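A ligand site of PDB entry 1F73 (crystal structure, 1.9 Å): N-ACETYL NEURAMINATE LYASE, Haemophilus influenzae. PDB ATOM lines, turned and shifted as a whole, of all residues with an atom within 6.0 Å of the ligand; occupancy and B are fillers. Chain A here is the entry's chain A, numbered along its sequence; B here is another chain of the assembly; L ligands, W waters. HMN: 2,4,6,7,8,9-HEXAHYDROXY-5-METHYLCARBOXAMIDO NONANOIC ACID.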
ATOM      1  N   ALA A  10      10.553 -16.857 -18.019  1.00  0.00           N
ATOM      2  CA  ALA A  10      10.052 -17.931 -18.885  1.00  0.00           C
ATOM      3  C   ALA A  10      11.139 -18.998 -18.775  1.00  0.00           C
ATOM      4  O   ALA A  10      12.209 -18.833 -19.373  1.00  0.00           O
ATOM      5  CB  ALA A  10       9.847 -17.428 -20.307  1.00  0.00           C
ATOM      6  N   LEU A  11      10.914 -20.008 -17.970  1.00  0.00           N
ATOM      7  CA  LEU A  11      11.858 -21.045 -17.676  1.00  0.00           C
ATOM      8  C   LEU A  11      12.458 -21.801 -18.862  1.00  0.00           C
ATOM      9  O   LEU A  11      11.776 -22.428 -19.683  1.00  0.00           O
ATOM     10  CB  LEU A  11      11.256 -22.006 -16.635  1.00  0.00           C
ATOM     11  CG  LEU A  11      12.181 -23.117 -16.150  1.00  0.00           C
ATOM     12  CD1 LEU A  11      13.304 -22.578 -15.222  1.00  0.00           C
ATOM     13  CD2 LEU A  11      11.447 -24.220 -15.407  1.00  0.00           C
ATOM     14  N   TYR A  43       7.376 -18.992 -15.366  1.00  0.00           N
ATOM     15  CA  TYR A  43       6.362 -19.327 -16.381  1.00  0.00           C
ATOM     16  C   TYR A  43       6.936 -20.548 -17.058  1.00  0.00           C
ATOM     17  O   TYR A  43       7.952 -20.496 -17.767  1.00  0.00           O
ATOM     18  CB  TYR A  43       6.195 -18.118 -17.283  1.00  0.00           C
ATOM     19  CG  TYR A  43       5.151 -18.177 -18.362  1.00  0.00           C
ATOM     20  CD1 TYR A  43       3.844 -17.784 -18.138  1.00  0.00           C
ATOM     21  CD2 TYR A  43       5.496 -18.643 -19.630  1.00  0.00           C
ATOM     22  CE1 TYR A  43       2.902 -17.848 -19.148  1.00  0.00           C
ATOM     23  CE2 TYR A  43       4.575 -18.710 -20.665  1.00  0.00           C
ATOM     24  CZ  TYR A  43       3.298 -18.291 -20.397  1.00  0.00           C
ATOM     25  OH  TYR A  43       2.382 -18.354 -21.424  1.00  0.00           O
ATOM     26  N   GLY A  45       6.955 -24.134 -19.245  1.00  0.00           N
ATOM     27  CA  GLY A  45       6.376 -24.799 -20.422  1.00  0.00           C
ATOM     28  C   GLY A  45       6.030 -23.815 -21.527  1.00  0.00           C
ATOM     29  O   GLY A  45       5.144 -24.083 -22.371  1.00  0.00           O
ATOM     30  N   GLY A  46       6.571 -22.607 -21.412  1.00  0.00           N
ATOM     31  CA  GLY A  46       6.344 -21.587 -22.417  1.00  0.00           C
ATOM     32  C   GLY A  46       7.231 -21.889 -23.621  1.00  0.00           C
ATOM     33  O   GLY A  46       8.053 -22.820 -23.617  1.00  0.00           O
ATOM     34  N   SER A  47       7.194 -21.063 -24.638  1.00  0.00           N
ATOM     35  CA  SER A  47       8.045 -21.298 -25.791  1.00  0.00           C
ATOM     36  C   SER A  47       9.528 -21.185 -25.399  1.00  0.00           C
ATOM     37  O   SER A  47      10.355 -21.854 -26.010  1.00  0.00           O
ATOM     38  CB  SER A  47       7.701 -20.362 -26.936  1.00  0.00           C
ATOM     39  OG  SER A  47       8.008 -19.035 -26.642  1.00  0.00           O
ATOM     40  N   THR A  48       9.844 -20.428 -24.344  1.00  0.00           N
ATOM     41  CA  THR A  48      11.265 -20.326 -23.932  1.00  0.00           C
ATOM     42  C   THR A  48      11.794 -21.662 -23.437  1.00  0.00           C
ATOM     43  O   THR A  48      12.996 -21.977 -23.569  1.00  0.00           O
ATOM     44  CB  THR A  48      11.440 -19.248 -22.865  1.00  0.00           C
ATOM     45  OG1 THR A  48      10.906 -18.026 -23.396  1.00  0.00           O
ATOM     46  CG2 THR A  48      12.925 -19.094 -22.540  1.00  0.00           C
ATOM     47  N   GLY A  49      10.904 -22.510 -22.929  1.00  0.00           N
ATOM     48  CA  GLY A  49      11.155 -23.829 -22.446  1.00  0.00           C
ATOM     49  C   GLY A  49      11.321 -24.885 -23.513  1.00  0.00           C
ATOM     50  O   GLY A  49      11.442 -26.068 -23.212  1.00  0.00           O
ATOM     51  N   GLN A  79       2.300 -23.116 -18.632  1.00  0.00           N
ATOM     52  CA  GLN A  79       1.804 -22.933 -20.007  1.00  0.00           C
ATOM     53  C   GLN A  79       1.435 -24.291 -20.549  1.00  0.00           C
ATOM     54  O   GLN A  79       2.285 -25.191 -20.649  1.00  0.00           O
ATOM     55  CB  GLN A  79       2.874 -22.298 -20.910  1.00  0.00           C
ATOM     56  CG  GLN A  79       2.304 -21.670 -22.164  1.00  0.00           C
ATOM     57  CD  GLN A  79       1.802 -22.659 -23.200  1.00  0.00           C
ATOM     58  OE1 GLN A  79       0.727 -22.505 -23.767  1.00  0.00           O
ATOM     59  NE2 GLN A  79       2.558 -23.742 -23.450  1.00  0.00           N
ATOM     60  N   TYR A 136      -2.803 -15.923 -24.517  1.00  0.00           N
ATOM     61  CA  TYR A 136      -1.787 -15.354 -25.374  1.00  0.00           C
ATOM     62  C   TYR A 136      -1.852 -15.977 -26.771  1.00  0.00           C
ATOM     63  O   TYR A 136      -2.355 -17.095 -26.910  1.00  0.00           O
ATOM     64  CB  TYR A 136      -0.372 -15.462 -24.846  1.00  0.00           C
ATOM     65  CG  TYR A 136       0.478 -16.670 -25.111  1.00  0.00           C
ATOM     66  CD1 TYR A 136       1.299 -16.755 -26.226  1.00  0.00           C
ATOM     67  CD2 TYR A 136       0.503 -17.719 -24.195  1.00  0.00           C
ATOM     68  CE1 TYR A 136       2.100 -17.865 -26.463  1.00  0.00           C
ATOM     69  CE2 TYR A 136       1.308 -18.833 -24.420  1.00  0.00           C
ATOM     70  CZ  TYR A 136       2.090 -18.886 -25.541  1.00  0.00           C
ATOM     71  OH  TYR A 136       2.875 -20.002 -25.710  1.00  0.00           O
ATOM     72  N   LYS A 164      -0.915 -12.285 -21.650  1.00  0.00           N
ATOM     73  CA  LYS A 164       0.516 -12.121 -21.817  1.00  0.00           C
ATOM     74  C   LYS A 164       0.655 -11.429 -23.194  1.00  0.00           C
ATOM     75  O   LYS A 164       0.477 -12.101 -24.205  1.00  0.00           O
ATOM     76  CB  LYS A 164       1.284 -13.406 -21.781  1.00  0.00           C
ATOM     77  CG  LYS A 164       2.795 -13.249 -22.038  1.00  0.00           C
ATOM     78  CD  LYS A 164       3.447 -14.631 -22.108  1.00  0.00           C
ATOM     79  CE  LYS A 164       3.181 -15.180 -23.537  1.00  0.00           C
ATOM     80  NZ  LYS A 164       3.790 -16.530 -23.690  1.00  0.00           N
ATOM     81  N   THR A 166       2.221 -10.001 -26.377  1.00  0.00           N
ATOM     82  CA  THR A 166       3.483 -10.329 -27.038  1.00  0.00           C
ATOM     83  C   THR A 166       3.725  -9.520 -28.297  1.00  0.00           C
ATOM     84  O   THR A 166       4.841  -9.556 -28.820  1.00  0.00           O
ATOM     85  CB  THR A 166       3.503 -11.829 -27.407  1.00  0.00           C
ATOM     86  OG1 THR A 166       2.286 -12.076 -28.138  1.00  0.00           O
ATOM     87  CG2 THR A 166       3.444 -12.740 -26.182  1.00  0.00           C
ATOM     88  N   ALA A 187       3.799  -7.985 -19.883  1.00  0.00           N
ATOM     89  CA  ALA A 187       4.491  -7.670 -21.149  1.00  0.00           C
ATOM     90  C   ALA A 187       5.356  -8.872 -21.482  1.00  0.00           C
ATOM     91  O   ALA A 187       5.954  -9.469 -20.587  1.00  0.00           O
ATOM     92  CB  ALA A 187       5.356  -6.426 -21.031  1.00  0.00           C
ATOM     93  N   GLY A 188       5.376  -9.276 -22.744  1.00  0.00           N
ATOM     94  CA  GLY A 188       6.176 -10.425 -23.145  1.00  0.00           C
ATOM     95  C   GLY A 188       7.489  -9.994 -23.783  1.00  0.00           C
ATOM     96  O   GLY A 188       8.309 -10.875 -24.047  1.00  0.00           O
ATOM     97  N   PHE A 189       7.685  -8.726 -24.077  1.00  0.00           N
ATOM     98  CA  PHE A 189       8.831  -8.207 -24.802  1.00  0.00           C
ATOM     99  C   PHE A 189       9.847  -7.510 -23.883  1.00  0.00           C
ATOM    100  O   PHE A 189       9.667  -6.367 -23.530  1.00  0.00           O
ATOM    101  CB  PHE A 189       8.370  -7.241 -25.899  1.00  0.00           C
ATOM    102  CG  PHE A 189       7.003  -6.647 -25.729  1.00  0.00           C
ATOM    103  CD1 PHE A 189       6.713  -5.696 -24.759  1.00  0.00           C
ATOM    104  CD2 PHE A 189       5.965  -7.050 -26.566  1.00  0.00           C
ATOM    105  CE1 PHE A 189       5.447  -5.168 -24.603  1.00  0.00           C
ATOM    106  CE2 PHE A 189       4.684  -6.519 -26.442  1.00  0.00           C
ATOM    107  CZ  PHE A 189       4.443  -5.565 -25.467  1.00  0.00           C
ATOM    108  N   ASP A 190      10.896  -8.210 -23.510  1.00  0.00           N
ATOM    109  CA  ASP A 190      11.872  -7.746 -22.532  1.00  0.00           C
ATOM    110  C   ASP A 190      12.499  -6.420 -22.922  1.00  0.00           C
ATOM    111  O   ASP A 190      12.706  -5.559 -22.082  1.00  0.00           O
ATOM    112  CB  ASP A 190      12.969  -8.806 -22.313  1.00  0.00           C
ATOM    113  CG  ASP A 190      12.472 -10.209 -22.033  1.00  0.00           C
ATOM    114  OD1 ASP A 190      11.295 -10.588 -22.322  1.00  0.00           O
ATOM    115  OD2 ASP A 190      13.321 -11.012 -21.559  1.00  0.00           O
ATOM    116  N   GLU A 191      12.810  -6.241 -24.202  1.00  0.00           N
ATOM    117  CA  GLU A 191      13.442  -5.068 -24.771  1.00  0.00           C
ATOM    118  C   GLU A 191      12.498  -3.898 -24.863  1.00  0.00           C
ATOM    119  O   GLU A 191      12.954  -2.810 -25.224  1.00  0.00           O
ATOM    120  CB  GLU A 191      14.088  -5.380 -26.130  1.00  0.00           C
ATOM    121  CG  GLU A 191      13.141  -5.945 -27.200  1.00  0.00           C
ATOM    122  CD  GLU A 191      13.047  -7.465 -27.133  1.00  0.00           C
ATOM    123  OE1 GLU A 191      12.825  -8.048 -26.061  1.00  0.00           O
ATOM    124  OE2 GLU A 191      13.204  -8.225 -28.114  1.00  0.00           O
ATOM    125  N   ILE A 205       6.757 -11.367 -18.493  1.00  0.00           N
ATOM    126  CA  ILE A 205       7.149 -12.784 -18.623  1.00  0.00           C
ATOM    127  C   ILE A 205       8.240 -12.782 -19.689  1.00  0.00           C
ATOM    128  O   ILE A 205       7.954 -12.327 -20.801  1.00  0.00           O
ATOM    129  CB  ILE A 205       5.951 -13.673 -19.025  1.00  0.00           C
ATOM    130  CG1 ILE A 205       4.949 -13.662 -17.879  1.00  0.00           C
ATOM    131  CG2 ILE A 205       6.393 -15.084 -19.340  1.00  0.00           C
ATOM    132  CD1 ILE A 205       3.576 -14.201 -18.144  1.00  0.00           C
ATOM    133  N   GLY A 206       9.477 -13.234 -19.387  1.00  0.00           N
ATOM    134  CA  GLY A 206      10.504 -13.020 -20.429  1.00  0.00           C
ATOM    135  C   GLY A 206      11.657 -13.990 -20.314  1.00  0.00           C
ATOM    136  O   GLY A 206      11.932 -14.491 -19.220  1.00  0.00           O
ATOM    137  N   SER A 207      12.282 -14.293 -21.463  1.00  0.00           N
ATOM    138  CA  SER A 207      13.373 -15.247 -21.437  1.00  0.00           C
ATOM    139  C   SER A 207      14.665 -14.632 -20.868  1.00  0.00           C
ATOM    140  O   SER A 207      15.379 -15.419 -20.233  1.00  0.00           O
ATOM    141  CB  SER A 207      13.743 -15.636 -22.888  1.00  0.00           C
ATOM    142  OG  SER A 207      14.007 -14.428 -23.595  1.00  0.00           O
ATOM    143  N   THR A 208      14.896 -13.359 -21.095  1.00  0.00           N
ATOM    144  CA  THR A 208      16.182 -12.766 -20.643  1.00  0.00           C
ATOM    145  C   THR A 208      16.275 -12.543 -19.134  1.00  0.00           C
ATOM    146  O   THR A 208      17.386 -12.366 -18.599  1.00  0.00           O
ATOM    147  CB  THR A 208      16.598 -11.513 -21.370  1.00  0.00           C
ATOM    148  OG1 THR A 208      15.823 -10.436 -20.876  1.00  0.00           O
ATOM    149  CG2 THR A 208      16.477 -11.582 -22.912  1.00  0.00           C
ATOM    150  N   ILE A 242      20.515  -7.603 -24.715  1.00  0.00           N
ATOM    151  CA  ILE A 242      19.525  -8.309 -25.552  1.00  0.00           C
ATOM    152  C   ILE A 242      19.853  -8.285 -27.033  1.00  0.00           C
ATOM    153  O   ILE A 242      19.761  -9.321 -27.697  1.00  0.00           O
ATOM    154  CB  ILE A 242      18.110  -7.707 -25.368  1.00  0.00           C
ATOM    155  CG1 ILE A 242      17.674  -7.870 -23.906  1.00  0.00           C
ATOM    156  CG2 ILE A 242      17.135  -8.456 -26.337  1.00  0.00           C
ATOM    157  CD1 ILE A 242      16.267  -7.326 -23.625  1.00  0.00           C
ATOM    158  N   LEU A 246      20.325 -11.675 -29.143  1.00  0.00           N
ATOM    159  CA  LEU A 246      19.582 -11.949 -30.348  1.00  0.00           C
ATOM    160  C   LEU A 246      20.463 -12.272 -31.550  1.00  0.00           C
ATOM    161  O   LEU A 246      20.276 -13.218 -32.298  1.00  0.00           O
ATOM    162  CB  LEU A 246      18.676 -10.733 -30.694  1.00  0.00           C
ATOM    163  CG  LEU A 246      17.516 -10.620 -29.651  1.00  0.00           C
ATOM    164  CD1 LEU A 246      16.827  -9.273 -29.777  1.00  0.00           C
ATOM    165  CD2 LEU A 246      16.565 -11.785 -29.852  1.00  0.00           C
ATOM    166  N   LEU A 250      19.409 -16.515 -29.571  1.00  0.00           N
ATOM    167  CA  LEU A 250      18.777 -16.393 -28.256  1.00  0.00           C
ATOM    168  C   LEU A 250      18.890 -17.559 -27.302  1.00  0.00           C
ATOM    169  O   LEU A 250      19.371 -17.403 -26.160  1.00  0.00           O
ATOM    170  CB  LEU A 250      17.280 -16.092 -28.481  1.00  0.00           C
ATOM    171  CG  LEU A 250      16.447 -15.929 -27.176  1.00  0.00           C
ATOM    172  CD1 LEU A 250      16.707 -14.553 -26.585  1.00  0.00           C
ATOM    173  CD2 LEU A 250      14.953 -16.038 -27.522  1.00  0.00           C
ATOM    174  N   TYR A 251      18.338 -18.732 -27.671  1.00  0.00           N
ATOM    175  CA  TYR A 251      18.298 -19.867 -26.742  1.00  0.00           C
ATOM    176  C   TYR A 251      19.688 -20.324 -26.312  1.00  0.00           C
ATOM    177  O   TYR A 251      19.951 -20.477 -25.123  1.00  0.00           O
ATOM    178  CB  TYR A 251      17.531 -21.056 -27.374  1.00  0.00           C
ATOM    179  CG  TYR A 251      16.084 -20.655 -27.626  1.00  0.00           C
ATOM    180  CD1 TYR A 251      15.159 -20.738 -26.597  1.00  0.00           C
ATOM    181  CD2 TYR A 251      15.673 -20.163 -28.851  1.00  0.00           C
ATOM    182  CE1 TYR A 251      13.854 -20.340 -26.793  1.00  0.00           C
ATOM    183  CE2 TYR A 251      14.368 -19.756 -29.053  1.00  0.00           C
ATOM    184  CZ  TYR A 251      13.466 -19.847 -28.020  1.00  0.00           C
ATOM    185  OH  TYR A 251      12.167 -19.450 -28.180  1.00  0.00           O
ATOM    186  N   TYR B 110       5.848 -23.192 -35.539  1.00  0.00           N
ATOM    187  CA  TYR B 110       5.756 -22.528 -34.249  1.00  0.00           C
ATOM    188  C   TYR B 110       7.003 -21.635 -34.151  1.00  0.00           C
ATOM    189  O   TYR B 110       6.884 -20.400 -34.268  1.00  0.00           O
ATOM    190  CB  TYR B 110       5.627 -23.422 -33.014  1.00  0.00           C
ATOM    191  CG  TYR B 110       5.300 -22.552 -31.811  1.00  0.00           C
ATOM    192  CD1 TYR B 110       3.986 -22.245 -31.478  1.00  0.00           C
ATOM    193  CD2 TYR B 110       6.325 -22.022 -31.054  1.00  0.00           C
ATOM    194  CE1 TYR B 110       3.715 -21.413 -30.396  1.00  0.00           C
ATOM    195  CE2 TYR B 110       6.072 -21.195 -29.981  1.00  0.00           C
ATOM    196  CZ  TYR B 110       4.762 -20.904 -29.654  1.00  0.00           C
ATOM    197  OH  TYR B 110       4.522 -20.058 -28.588  1.00  0.00           O
HETATM  198  C1  HMN L   1       7.381 -17.851 -23.332  1.00  0.00           C
HETATM  199  O1A HMN L   1       8.345 -18.635 -23.080  1.00  0.00           O
HETATM  200  O1B HMN L   1       6.205 -18.236 -23.592  1.00  0.00           O
HETATM  201  C2  HMN L   1       7.641 -16.372 -23.271  1.00  0.00           C
HETATM  202  O2  HMN L   1       6.449 -15.611 -23.035  1.00  0.00           O
HETATM  203  C3  HMN L   1       8.348 -15.891 -24.512  1.00  0.00           C
HETATM  204  C4  HMN L   1       8.934 -14.509 -24.223  1.00  0.00           C
HETATM  205  O4  HMN L   1       7.911 -13.545 -24.328  1.00  0.00           O
HETATM  206  C5  HMN L   1      10.046 -14.218 -25.233  1.00  0.00           C
HETATM  207  N2  HMN L   1       9.387 -14.203 -26.558  1.00  0.00           N
HETATM  208  C10 HMN L   1       9.902 -14.946 -27.548  1.00  0.00           C
HETATM  209  O10 HMN L   1      11.061 -15.370 -27.493  1.00  0.00           O
HETATM  210  C11 HMN L   1       9.063 -15.233 -28.775  1.00  0.00           C
HETATM  211  C6  HMN L   1      10.709 -12.853 -25.011  1.00  0.00           C
HETATM  212  O6  HMN L   1      11.197 -12.749 -23.682  1.00  0.00           O
HETATM  213  C7  HMN L   1      11.867 -12.685 -25.992  1.00  0.00           C
HETATM  214  O7  HMN L   1      12.761 -13.801 -25.966  1.00  0.00           O
HETATM  215  C8  HMN L   1      12.663 -11.432 -25.645  1.00  0.00           C
HETATM  216  O8  HMN L   1      11.755 -10.352 -25.654  1.00  0.00           O
HETATM  217  C9  HMN L   1      13.717 -11.289 -26.729  1.00  0.00           C
HETATM  218  O9  HMN L   1      13.168 -10.785 -27.937  1.00  0.00           O
HETATM  219  O   HOH W   1       9.542 -10.221 -27.514  1.00  0.00           O
HETATM  220  O   HOH W   2      10.573 -18.073 -26.365  1.00  0.00           O
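Merely in contact with the ligand: Ala 10, Tyr 43, Gly 46, Phe 189, Ile 205, Gly 206 and Leu 250.
Hydrophobic or aromatic side chains within 4 Å of the ligand: Ala 10, Tyr 43, Ile 205 and Leu 250.
14 residues have an atom within 4 Å of the ligand: Ala 10, Tyr 43, Gly 46, Ser 47, Thr 48, Lys 164, Gly 188, Phe 189, Asp 190, Glu 191, Ile 205, Gly 206, Ser 207 and Leu 250.
The nearest printed residue that does not touch the ligand is Leu 246 (4.03 Å).
N of Asp 190 is in hydrogen-bond range of O8 of the ligand, at 3.2 Å.
O6 of the ligand is in hydrogen-bond range of OD1 of Asp 190, at 2.6 Å.
An oxygen (O9) of the ligand lies within hydrogen-bond range of the side-chain carboxylate (OE2) of Glu 191 (2.6 Å).
N of Thr 48 sits at hydrogen-bond distance from O1A of the ligand.
O1A of the ligand lies within hydrogen-bond range of OG1 of Thr 48, 2.7 Å away.
The backbone carbonyl oxygen (O) of Gly 188 sits at hydrogen-bond distance from an oxygen (O4) of the ligand, at 2.7 Å.
N of Ser 207 lies within hydrogen-bond range of O6 of the ligand, 2.9 Å away.
The side-chain hydroxyl (OG) of Ser 207 lies within hydrogen-bond range of an oxygen (O7) of the ligand.
NZ of Lys 164 is in salt-bridge range of O1B of the ligand (3.0 Å).
An oxygen (O1A) of the ligand lies within hydrogen-bond range of the backbone NH of Ser 47, at 3.1 Å.
Water W2 lies within hydrogen-bond range of the side-chain hydroxyl (OG) of Ser 47, the side-chain hydroxyl (OH) of Tyr 251, an oxygen (O10) of the ligand and the side-chain hydroxyl (OG1) of Thr 48.
The side-chain carboxylate (OD2) of Asp 190 lies within hydrogen-bond range of the backbone NH (N) of Ser 207 (3.4 Å).
The side-chain carboxylate (OD2) of Asp 190 sits at hydrogen-bond distance from the side-chain hydroxyl (OG1) of Thr 208 (2.7 Å).
The side-chain amino group (NZ) of Lys 164 is in hydrogen-bond range of the side-chain hydroxyl (OH) of Tyr 43 (3.2 Å).
N of Ala 10 lies within hydrogen-bond range of O of Gly 206 (3.0 Å).
The backbone carbonyl oxygen (O) of Tyr 43 lies within hydrogen-bond range of the backbone NH (N) of Leu 11 (3.0 Å).
The backbone carbonyl oxygen (O) of Ala 187 lies within hydrogen-bond range of the backbone NH (N) of Ile 205 (2.9 Å).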
